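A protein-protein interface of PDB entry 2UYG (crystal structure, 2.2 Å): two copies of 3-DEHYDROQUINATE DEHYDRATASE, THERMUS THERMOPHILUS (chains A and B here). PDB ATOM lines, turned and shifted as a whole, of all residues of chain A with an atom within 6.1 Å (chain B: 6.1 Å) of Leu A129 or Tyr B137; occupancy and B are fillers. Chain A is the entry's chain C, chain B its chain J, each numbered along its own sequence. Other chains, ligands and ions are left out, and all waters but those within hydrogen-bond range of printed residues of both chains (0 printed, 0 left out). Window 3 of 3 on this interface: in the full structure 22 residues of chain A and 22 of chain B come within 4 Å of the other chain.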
ATOM      1  N   TRP A  36      -0.263  22.212  -9.860  1.00  0.00           N
ATOM      2  CA  TRP A  36       0.281  21.379  -8.786  1.00  0.00           C
ATOM      3  C   TRP A  36       1.751  21.716  -8.630  1.00  0.00           C
ATOM      4  O   TRP A  36       2.305  21.778  -7.524  1.00  0.00           O
ATOM      5  CB  TRP A  36       0.056  19.896  -9.062  1.00  0.00           C
ATOM      6  CG  TRP A  36      -1.333  19.429  -8.863  1.00  0.00           C
ATOM      7  CD1 TRP A  36      -2.257  19.869  -7.929  1.00  0.00           C
ATOM      8  CD2 TRP A  36      -2.001  18.397  -9.615  1.00  0.00           C
ATOM      9  NE1 TRP A  36      -3.428  19.149  -8.047  1.00  0.00           N
ATOM     10  CE2 TRP A  36      -3.284  18.229  -9.060  1.00  0.00           C
ATOM     11  CE3 TRP A  36      -1.617  17.560 -10.678  1.00  0.00           C
ATOM     12  CZ2 TRP A  36      -4.208  17.313  -9.587  1.00  0.00           C
ATOM     13  CZ3 TRP A  36      -2.525  16.614 -11.170  1.00  0.00           C
ATOM     14  CH2 TRP A  36      -3.797  16.502 -10.628  1.00  0.00           C
ATOM     15  N   LEU A 100      -2.556   6.577 -15.496  1.00  0.00           N
ATOM     16  CA  LEU A 100      -3.806   7.008 -14.935  1.00  0.00           C
ATOM     17  C   LEU A 100      -4.535   5.862 -14.254  1.00  0.00           C
ATOM     18  O   LEU A 100      -5.089   6.040 -13.147  1.00  0.00           O
ATOM     19  CB  LEU A 100      -4.651   7.684 -16.033  1.00  0.00           C
ATOM     20  CG  LEU A 100      -4.119   8.982 -16.669  1.00  0.00           C
ATOM     21  CD1 LEU A 100      -4.679   9.242 -18.085  1.00  0.00           C
ATOM     22  CD2 LEU A 100      -4.433  10.142 -15.846  1.00  0.00           C
ATOM     23  N   VAL A 123       4.054   5.327 -10.300  1.00  0.00           N
ATOM     24  CA  VAL A 123       2.798   5.493  -9.698  1.00  0.00           C
ATOM     25  C   VAL A 123       1.646   5.256 -10.681  1.00  0.00           C
ATOM     26  O   VAL A 123       1.568   5.851 -11.786  1.00  0.00           O
ATOM     27  CB  VAL A 123       2.660   6.854  -8.894  1.00  0.00           C
ATOM     28  CG1 VAL A 123       3.757   7.791  -9.114  1.00  0.00           C
ATOM     29  CG2 VAL A 123       1.308   7.455  -9.095  1.00  0.00           C
ATOM     30  N   GLY A 125      -2.829   4.319 -11.131  1.00  0.00           N
ATOM     31  CA  GLY A 125      -4.176   3.961 -10.773  1.00  0.00           C
ATOM     32  C   GLY A 125      -4.947   5.126 -10.207  1.00  0.00           C
ATOM     33  O   GLY A 125      -6.137   4.983  -9.985  1.00  0.00           O
ATOM     34  N   PHE A 126      -4.308   6.293 -10.047  1.00  0.00           N
ATOM     35  CA  PHE A 126      -4.937   7.400  -9.319  1.00  0.00           C
ATOM     36  C   PHE A 126      -5.575   8.432 -10.175  1.00  0.00           C
ATOM     37  O   PHE A 126      -5.857   9.464  -9.666  1.00  0.00           O
ATOM     38  CB  PHE A 126      -3.871   8.048  -8.405  1.00  0.00           C
ATOM     39  CG  PHE A 126      -3.203   7.058  -7.524  1.00  0.00           C
ATOM     40  CD1 PHE A 126      -1.886   6.641  -7.784  1.00  0.00           C
ATOM     41  CD2 PHE A 126      -3.898   6.510  -6.458  1.00  0.00           C
ATOM     42  CE1 PHE A 126      -1.257   5.757  -6.993  1.00  0.00           C
ATOM     43  CE2 PHE A 126      -3.300   5.561  -5.660  1.00  0.00           C
ATOM     44  CZ  PHE A 126      -1.958   5.160  -5.938  1.00  0.00           C
ATOM     45  N   GLY A 127      -5.847   8.136 -11.464  1.00  0.00           N
ATOM     46  CA  GLY A 127      -6.335   9.092 -12.444  1.00  0.00           C
ATOM     47  C   GLY A 127      -5.278  10.199 -12.599  1.00  0.00           C
ATOM     48  O   GLY A 127      -4.077   9.989 -12.464  1.00  0.00           O
ATOM     49  N   PRO A 128      -5.735  11.408 -12.878  1.00  0.00           N
ATOM     50  CA  PRO A 128      -4.886  12.629 -12.857  1.00  0.00           C
ATOM     51  C   PRO A 128      -3.939  12.808 -11.664  1.00  0.00           C
ATOM     52  O   PRO A 128      -2.819  13.357 -11.809  1.00  0.00           O
ATOM     53  CB  PRO A 128      -5.929  13.739 -12.866  1.00  0.00           C
ATOM     54  CG  PRO A 128      -7.027  13.074 -13.727  1.00  0.00           C
ATOM     55  CD  PRO A 128      -7.129  11.699 -13.248  1.00  0.00           C
ATOM     56  N   LEU A 129      -4.388  12.348 -10.490  1.00  0.00           N
ATOM     57  CA  LEU A 129      -3.578  12.459  -9.266  1.00  0.00           C
ATOM     58  C   LEU A 129      -2.273  11.665  -9.277  1.00  0.00           C
ATOM     59  O   LEU A 129      -1.400  11.905  -8.452  1.00  0.00           O
ATOM     60  CB  LEU A 129      -4.420  12.051  -8.044  1.00  0.00           C
ATOM     61  CG  LEU A 129      -5.471  13.100  -7.645  1.00  0.00           C
ATOM     62  CD1 LEU A 129      -6.312  12.545  -6.547  1.00  0.00           C
ATOM     63  CD2 LEU A 129      -4.825  14.396  -7.163  1.00  0.00           C
ATOM     64  N   SER A 130      -2.140  10.673 -10.179  1.00  0.00           N
ATOM     65  CA  SER A 130      -0.811  10.035 -10.351  1.00  0.00           C
ATOM     66  C   SER A 130       0.276  11.067 -10.683  1.00  0.00           C
ATOM     67  O   SER A 130       1.435  10.923 -10.295  1.00  0.00           O
ATOM     68  CB  SER A 130      -0.844   9.012 -11.487  1.00  0.00           C
ATOM     69  OG  SER A 130      -1.664   7.919 -11.161  1.00  0.00           O
ATOM     70  N   TYR A 131      -0.079  12.054 -11.495  1.00  0.00           N
ATOM     71  CA  TYR A 131       0.874  13.039 -11.934  1.00  0.00           C
ATOM     72  C   TYR A 131       1.277  13.904 -10.742  1.00  0.00           C
ATOM     73  O   TYR A 131       2.446  14.332 -10.618  1.00  0.00           O
ATOM     74  CB  TYR A 131       0.290  13.897 -13.030  1.00  0.00           C
ATOM     75  CG  TYR A 131       0.164  13.161 -14.392  1.00  0.00           C
ATOM     76  CD1 TYR A 131      -0.755  12.144 -14.590  1.00  0.00           C
ATOM     77  CD2 TYR A 131       0.962  13.523 -15.482  1.00  0.00           C
ATOM     78  CE1 TYR A 131      -0.841  11.474 -15.849  1.00  0.00           C
ATOM     79  CE2 TYR A 131       0.905  12.808 -16.757  1.00  0.00           C
ATOM     80  CZ  TYR A 131       0.010  11.819 -16.891  1.00  0.00           C
ATOM     81  OH  TYR A 131      -0.103  11.200 -18.093  1.00  0.00           O
ATOM     82  N   LYS A 132       0.296  14.164  -9.880  1.00  0.00           N
ATOM     83  CA  LYS A 132       0.490  15.027  -8.770  1.00  0.00           C
ATOM     84  C   LYS A 132       1.378  14.327  -7.808  1.00  0.00           C
ATOM     85  O   LYS A 132       2.300  14.934  -7.357  1.00  0.00           O
ATOM     86  CB  LYS A 132      -0.785  15.407  -8.096  1.00  0.00           C
ATOM     87  CG  LYS A 132      -0.519  16.586  -7.189  1.00  0.00           C
ATOM     88  CD  LYS A 132      -1.007  16.333  -5.867  1.00  0.00           C
ATOM     89  CE  LYS A 132      -2.230  17.192  -5.506  1.00  0.00           C
ATOM     90  NZ  LYS A 132      -1.931  17.941  -4.156  1.00  0.00           N
ATOM     91  N   LEU A 133       1.159  13.055  -7.532  1.00  0.00           N
ATOM     92  CA  LEU A 133       2.055  12.358  -6.667  1.00  0.00           C
ATOM     93  C   LEU A 133       3.531  12.384  -7.084  1.00  0.00           C
ATOM     94  O   LEU A 133       4.447  12.468  -6.237  1.00  0.00           O
ATOM     95  CB  LEU A 133       1.607  10.937  -6.476  1.00  0.00           C
ATOM     96  CG  LEU A 133       0.206  10.613  -5.963  1.00  0.00           C
ATOM     97  CD1 LEU A 133       0.148   9.292  -5.172  1.00  0.00           C
ATOM     98  CD2 LEU A 133      -0.584  11.719  -5.208  1.00  0.00           C
ATOM     99  N   ALA A 134       3.756  12.281  -8.377  1.00  0.00           N
ATOM    100  CA  ALA A 134       5.095  12.352  -8.955  1.00  0.00           C
ATOM    101  C   ALA A 134       5.723  13.704  -8.745  1.00  0.00           C
ATOM    102  O   ALA A 134       6.917  13.785  -8.515  1.00  0.00           O
ATOM    103  CB  ALA A 134       5.031  12.088 -10.488  1.00  0.00           C
ATOM    104  N   PRO B  94     -11.030   1.577   0.097  1.00  0.00           N
ATOM    105  CA  PRO B  94      -9.934   1.693  -0.866  1.00  0.00           C
ATOM    106  C   PRO B  94      -8.647   1.266  -0.216  1.00  0.00           C
ATOM    107  O   PRO B  94      -8.417   1.555   0.912  1.00  0.00           O
ATOM    108  CB  PRO B  94      -9.897   3.196  -1.184  1.00  0.00           C
ATOM    109  CG  PRO B  94     -10.610   3.823  -0.076  1.00  0.00           C
ATOM    110  CD  PRO B  94     -11.661   2.876   0.384  1.00  0.00           C
ATOM    111  N   VAL B  96      -4.479   1.334  -1.096  1.00  0.00           N
ATOM    112  CA  VAL B  96      -3.358   1.741  -1.922  1.00  0.00           C
ATOM    113  C   VAL B  96      -2.210   0.829  -1.587  1.00  0.00           C
ATOM    114  O   VAL B  96      -1.836   0.722  -0.379  1.00  0.00           O
ATOM    115  CB  VAL B  96      -2.938   3.138  -1.637  1.00  0.00           C
ATOM    116  CG1 VAL B  96      -1.838   3.571  -2.534  1.00  0.00           C
ATOM    117  CG2 VAL B  96      -4.114   4.077  -1.830  1.00  0.00           C
ATOM    118  N   ARG B 120      -6.801   0.346  -5.423  1.00  0.00           N
ATOM    119  CA  ARG B 120      -7.043   1.579  -6.148  1.00  0.00           C
ATOM    120  C   ARG B 120      -5.864   1.841  -7.046  1.00  0.00           C
ATOM    121  O   ARG B 120      -6.038   2.214  -8.191  1.00  0.00           O
ATOM    122  CB  ARG B 120      -7.053   2.762  -5.206  1.00  0.00           C
ATOM    123  CG  ARG B 120      -8.293   3.490  -4.984  1.00  0.00           C
ATOM    124  CD  ARG B 120      -9.277   3.848  -6.154  1.00  0.00           C
ATOM    125  NE  ARG B 120     -10.498   3.363  -5.502  1.00  0.00           N
ATOM    126  CZ  ARG B 120     -11.469   4.055  -4.906  1.00  0.00           C
ATOM    127  NH1 ARG B 120     -12.457   3.383  -4.298  1.00  0.00           N
ATOM    128  NH2 ARG B 120     -11.530   5.378  -4.955  1.00  0.00           N
ATOM    129  N   LYS B 132       4.184   8.621   1.787  1.00  0.00           N
ATOM    130  CA  LYS B 132       3.644   9.910   1.663  1.00  0.00           C
ATOM    131  C   LYS B 132       2.771  10.130   0.451  1.00  0.00           C
ATOM    132  O   LYS B 132       1.737  10.869   0.543  1.00  0.00           O
ATOM    133  CB  LYS B 132       4.728  10.913   1.654  1.00  0.00           C
ATOM    134  CG  LYS B 132       4.148  12.247   1.990  1.00  0.00           C
ATOM    135  CD  LYS B 132       4.875  13.330   1.203  1.00  0.00           C
ATOM    136  CE  LYS B 132       5.808  14.146   2.005  1.00  0.00           C
ATOM    137  NZ  LYS B 132       5.420  15.548   1.999  1.00  0.00           N
ATOM    138  N   LEU B 133       3.141   9.577  -0.723  1.00  0.00           N
ATOM    139  CA  LEU B 133       2.309   9.874  -1.904  1.00  0.00           C
ATOM    140  C   LEU B 133       1.021   9.140  -1.692  1.00  0.00           C
ATOM    141  O   LEU B 133      -0.006   9.620  -2.015  1.00  0.00           O
ATOM    142  CB  LEU B 133       2.952   9.578  -3.297  1.00  0.00           C
ATOM    143  CG  LEU B 133       4.424   9.824  -3.582  1.00  0.00           C
ATOM    144  CD1 LEU B 133       4.882   9.313  -5.005  1.00  0.00           C
ATOM    145  CD2 LEU B 133       4.781  11.239  -3.288  1.00  0.00           C
ATOM    146  N   ALA B 134       1.051   7.982  -1.128  1.00  0.00           N
ATOM    147  CA  ALA B 134      -0.209   7.315  -0.843  1.00  0.00           C
ATOM    148  C   ALA B 134      -1.129   8.273   0.008  1.00  0.00           C
ATOM    149  O   ALA B 134      -2.344   8.361  -0.233  1.00  0.00           O
ATOM    150  CB  ALA B 134       0.059   6.051  -0.062  1.00  0.00           C
ATOM    151  N   LEU B 135      -0.538   8.932   1.031  1.00  0.00           N
ATOM    152  CA  LEU B 135      -1.350   9.731   1.918  1.00  0.00           C
ATOM    153  C   LEU B 135      -1.866  11.001   1.212  1.00  0.00           C
ATOM    154  O   LEU B 135      -2.936  11.433   1.500  1.00  0.00           O
ATOM    155  CB  LEU B 135      -0.659   9.999   3.264  1.00  0.00           C
ATOM    156  CG  LEU B 135      -0.267   8.766   4.050  1.00  0.00           C
ATOM    157  CD1 LEU B 135       0.752   9.103   5.106  1.00  0.00           C
ATOM    158  CD2 LEU B 135      -1.423   8.146   4.661  1.00  0.00           C
ATOM    159  N   VAL B 136      -1.169  11.569   0.247  1.00  0.00           N
ATOM    160  CA  VAL B 136      -1.715  12.750  -0.368  1.00  0.00           C
ATOM    161  C   VAL B 136      -2.851  12.367  -1.300  1.00  0.00           C
ATOM    162  O   VAL B 136      -3.843  13.083  -1.406  1.00  0.00           O
ATOM    163  CB  VAL B 136      -0.664  13.711  -1.008  1.00  0.00           C
ATOM    164  CG1 VAL B 136       0.665  13.157  -0.957  1.00  0.00           C
ATOM    165  CG2 VAL B 136      -1.103  14.203  -2.411  1.00  0.00           C
ATOM    166  N   TYR B 137      -2.773  11.202  -1.931  1.00  0.00           N
ATOM    167  CA  TYR B 137      -3.881  10.841  -2.816  1.00  0.00           C
ATOM    168  C   TYR B 137      -5.143  10.668  -1.905  1.00  0.00           C
ATOM    169  O   TYR B 137      -6.212  11.147  -2.171  1.00  0.00           O
ATOM    170  CB  TYR B 137      -3.589   9.529  -3.570  1.00  0.00           C
ATOM    171  CG  TYR B 137      -4.846   8.904  -4.068  1.00  0.00           C
ATOM    172  CD1 TYR B 137      -5.518   9.462  -5.142  1.00  0.00           C
ATOM    173  CD2 TYR B 137      -5.389   7.785  -3.454  1.00  0.00           C
ATOM    174  CE1 TYR B 137      -6.700   8.911  -5.633  1.00  0.00           C
ATOM    175  CE2 TYR B 137      -6.569   7.200  -3.952  1.00  0.00           C
ATOM    176  CZ  TYR B 137      -7.190   7.777  -5.056  1.00  0.00           C
ATOM    177  OH  TYR B 137      -8.355   7.296  -5.507  1.00  0.00           O
ATOM    178  N   LEU B 138      -4.969   9.907  -0.854  1.00  0.00           N
ATOM    179  CA  LEU B 138      -6.021   9.606   0.081  1.00  0.00           C
ATOM    180  C   LEU B 138      -6.637  10.858   0.716  1.00  0.00           C
ATOM    181  O   LEU B 138      -7.853  10.877   0.896  1.00  0.00           O
ATOM    182  CB  LEU B 138      -5.505   8.660   1.172  1.00  0.00           C
ATOM    183  CG  LEU B 138      -5.909   7.154   1.160  1.00  0.00           C
ATOM    184  CD1 LEU B 138      -6.377   6.685  -0.092  1.00  0.00           C
ATOM    185  CD2 LEU B 138      -4.761   6.239   1.691  1.00  0.00           C
ATOM    186  N   ALA B 139      -5.819  11.894   0.992  1.00  0.00           N
ATOM    187  CA  ALA B 139      -6.317  13.143   1.619  1.00  0.00           C
ATOM    188  C   ALA B 139      -7.302  13.836   0.725  1.00  0.00           C
ATOM    189  O   ALA B 139      -8.369  14.241   1.187  1.00  0.00           O
ATOM    190  CB  ALA B 139      -5.235  14.075   1.893  1.00  0.00           C
ATOM    191  N   GLU B 140      -6.936  13.923  -0.562  1.00  0.00           N
ATOM    192  CA  GLU B 140      -7.755  14.582  -1.576  1.00  0.00           C
ATOM    193  C   GLU B 140      -9.107  13.885  -1.837  1.00  0.00           C
ATOM    194  O   GLU B 140     -10.125  14.521  -2.075  1.00  0.00           O
ATOM    195  CB  GLU B 140      -6.965  14.650  -2.859  1.00  0.00           C
ATOM    196  CG  GLU B 140      -7.502  15.689  -3.797  1.00  0.00           C
ATOM    197  CD  GLU B 140      -6.412  16.513  -4.427  1.00  0.00           C
ATOM    198  OE1 GLU B 140      -5.249  16.528  -3.898  1.00  0.00           O
ATOM    199  OE2 GLU B 140      -6.761  17.145  -5.445  1.00  0.00           O
ATOM    200  N   THR B 141      -9.116  12.573  -1.719  1.00  0.00           N
ATOM    201  CA  THR B 141     -10.191  11.748  -2.218  1.00  0.00           C
ATOM    202  C   THR B 141     -11.221  11.424  -1.129  1.00  0.00           C
ATOM    203  O   THR B 141     -10.915  11.554   0.083  1.00  0.00           O
ATOM    204  CB  THR B 141      -9.506  10.477  -2.675  1.00  0.00           C
ATOM    205  OG1 THR B 141      -8.382  10.863  -3.484  1.00  0.00           O
ATOM    206  CG2 THR B 141     -10.367   9.652  -3.577  1.00  0.00           C
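The backbone carbonyl oxygen of Arg B120 sits close to the backbone carbonyl oxygen of Gly A125, at 3.3 Å. OE1 of Glu B140 lies within salt-bridge range of NZ of Lys A132, at 3.6 Å.
The backbone carbonyl oxygen of Tyr B137 is in hydrogen-bond range of the side-chain hydroxyl of Thr B141, at 2.6 Å. The backbone carbonyl oxygen (O) of Leu A100 lies within hydrogen-bond range of the backbone NH (N) of Phe A126 (3.2 Å). The backbone carbonyl oxygen of Leu A100 sits close to the backbone NH of Gly A125, at 3.5 Å. The side-chain hydroxyl (OG) of Ser A130 lies within hydrogen-bond range of the backbone NH (N) of Phe A126 (3.3 Å).
Phe A126 touches Val B96 (CZ to CG1, 3.8 Å). Phe A126 touches Tyr B137 (CD2 to CG, 3.5 Å). Leu A129 touches Tyr B137. OE2 of Glu B140 touches CD2 of Leu A129 (3.8 Å). Leu A133 touches Leu B133. CG2 of Val B136 touches CD2 of Leu A133 (3.8 Å). Leu A133 touches Tyr B137.
Of the printed residues of chain B, Phe A126 touches Val B96 and Tyr B137. Of the printed residues of chain B, Leu A133 touches Leu B133 (3.2 Å), Val B136 (3.8 Å) and Tyr B137 (3.97 Å). Of the printed residues of chain A, Val B96 touches Phe A126. Lys B132 touches none of the printed residues of chain A. Of chain A, only Phe A126, Leu A129 and Leu A133 come within 4 Å of Tyr B137. The nearest residue of chain A that does not touch Tyr B137 is Gly A125 (5.5 Å).
Hydrophobic or aromatic side chains of chain A that line the printed part of chain B: Phe A126, Leu A129 and Leu A133. Among the printed residues, 9 pairs touch across the chains.
Leu B133 touches its own counterpart, Leu A133. Positions printed for both chains: 132, 133 and 134.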
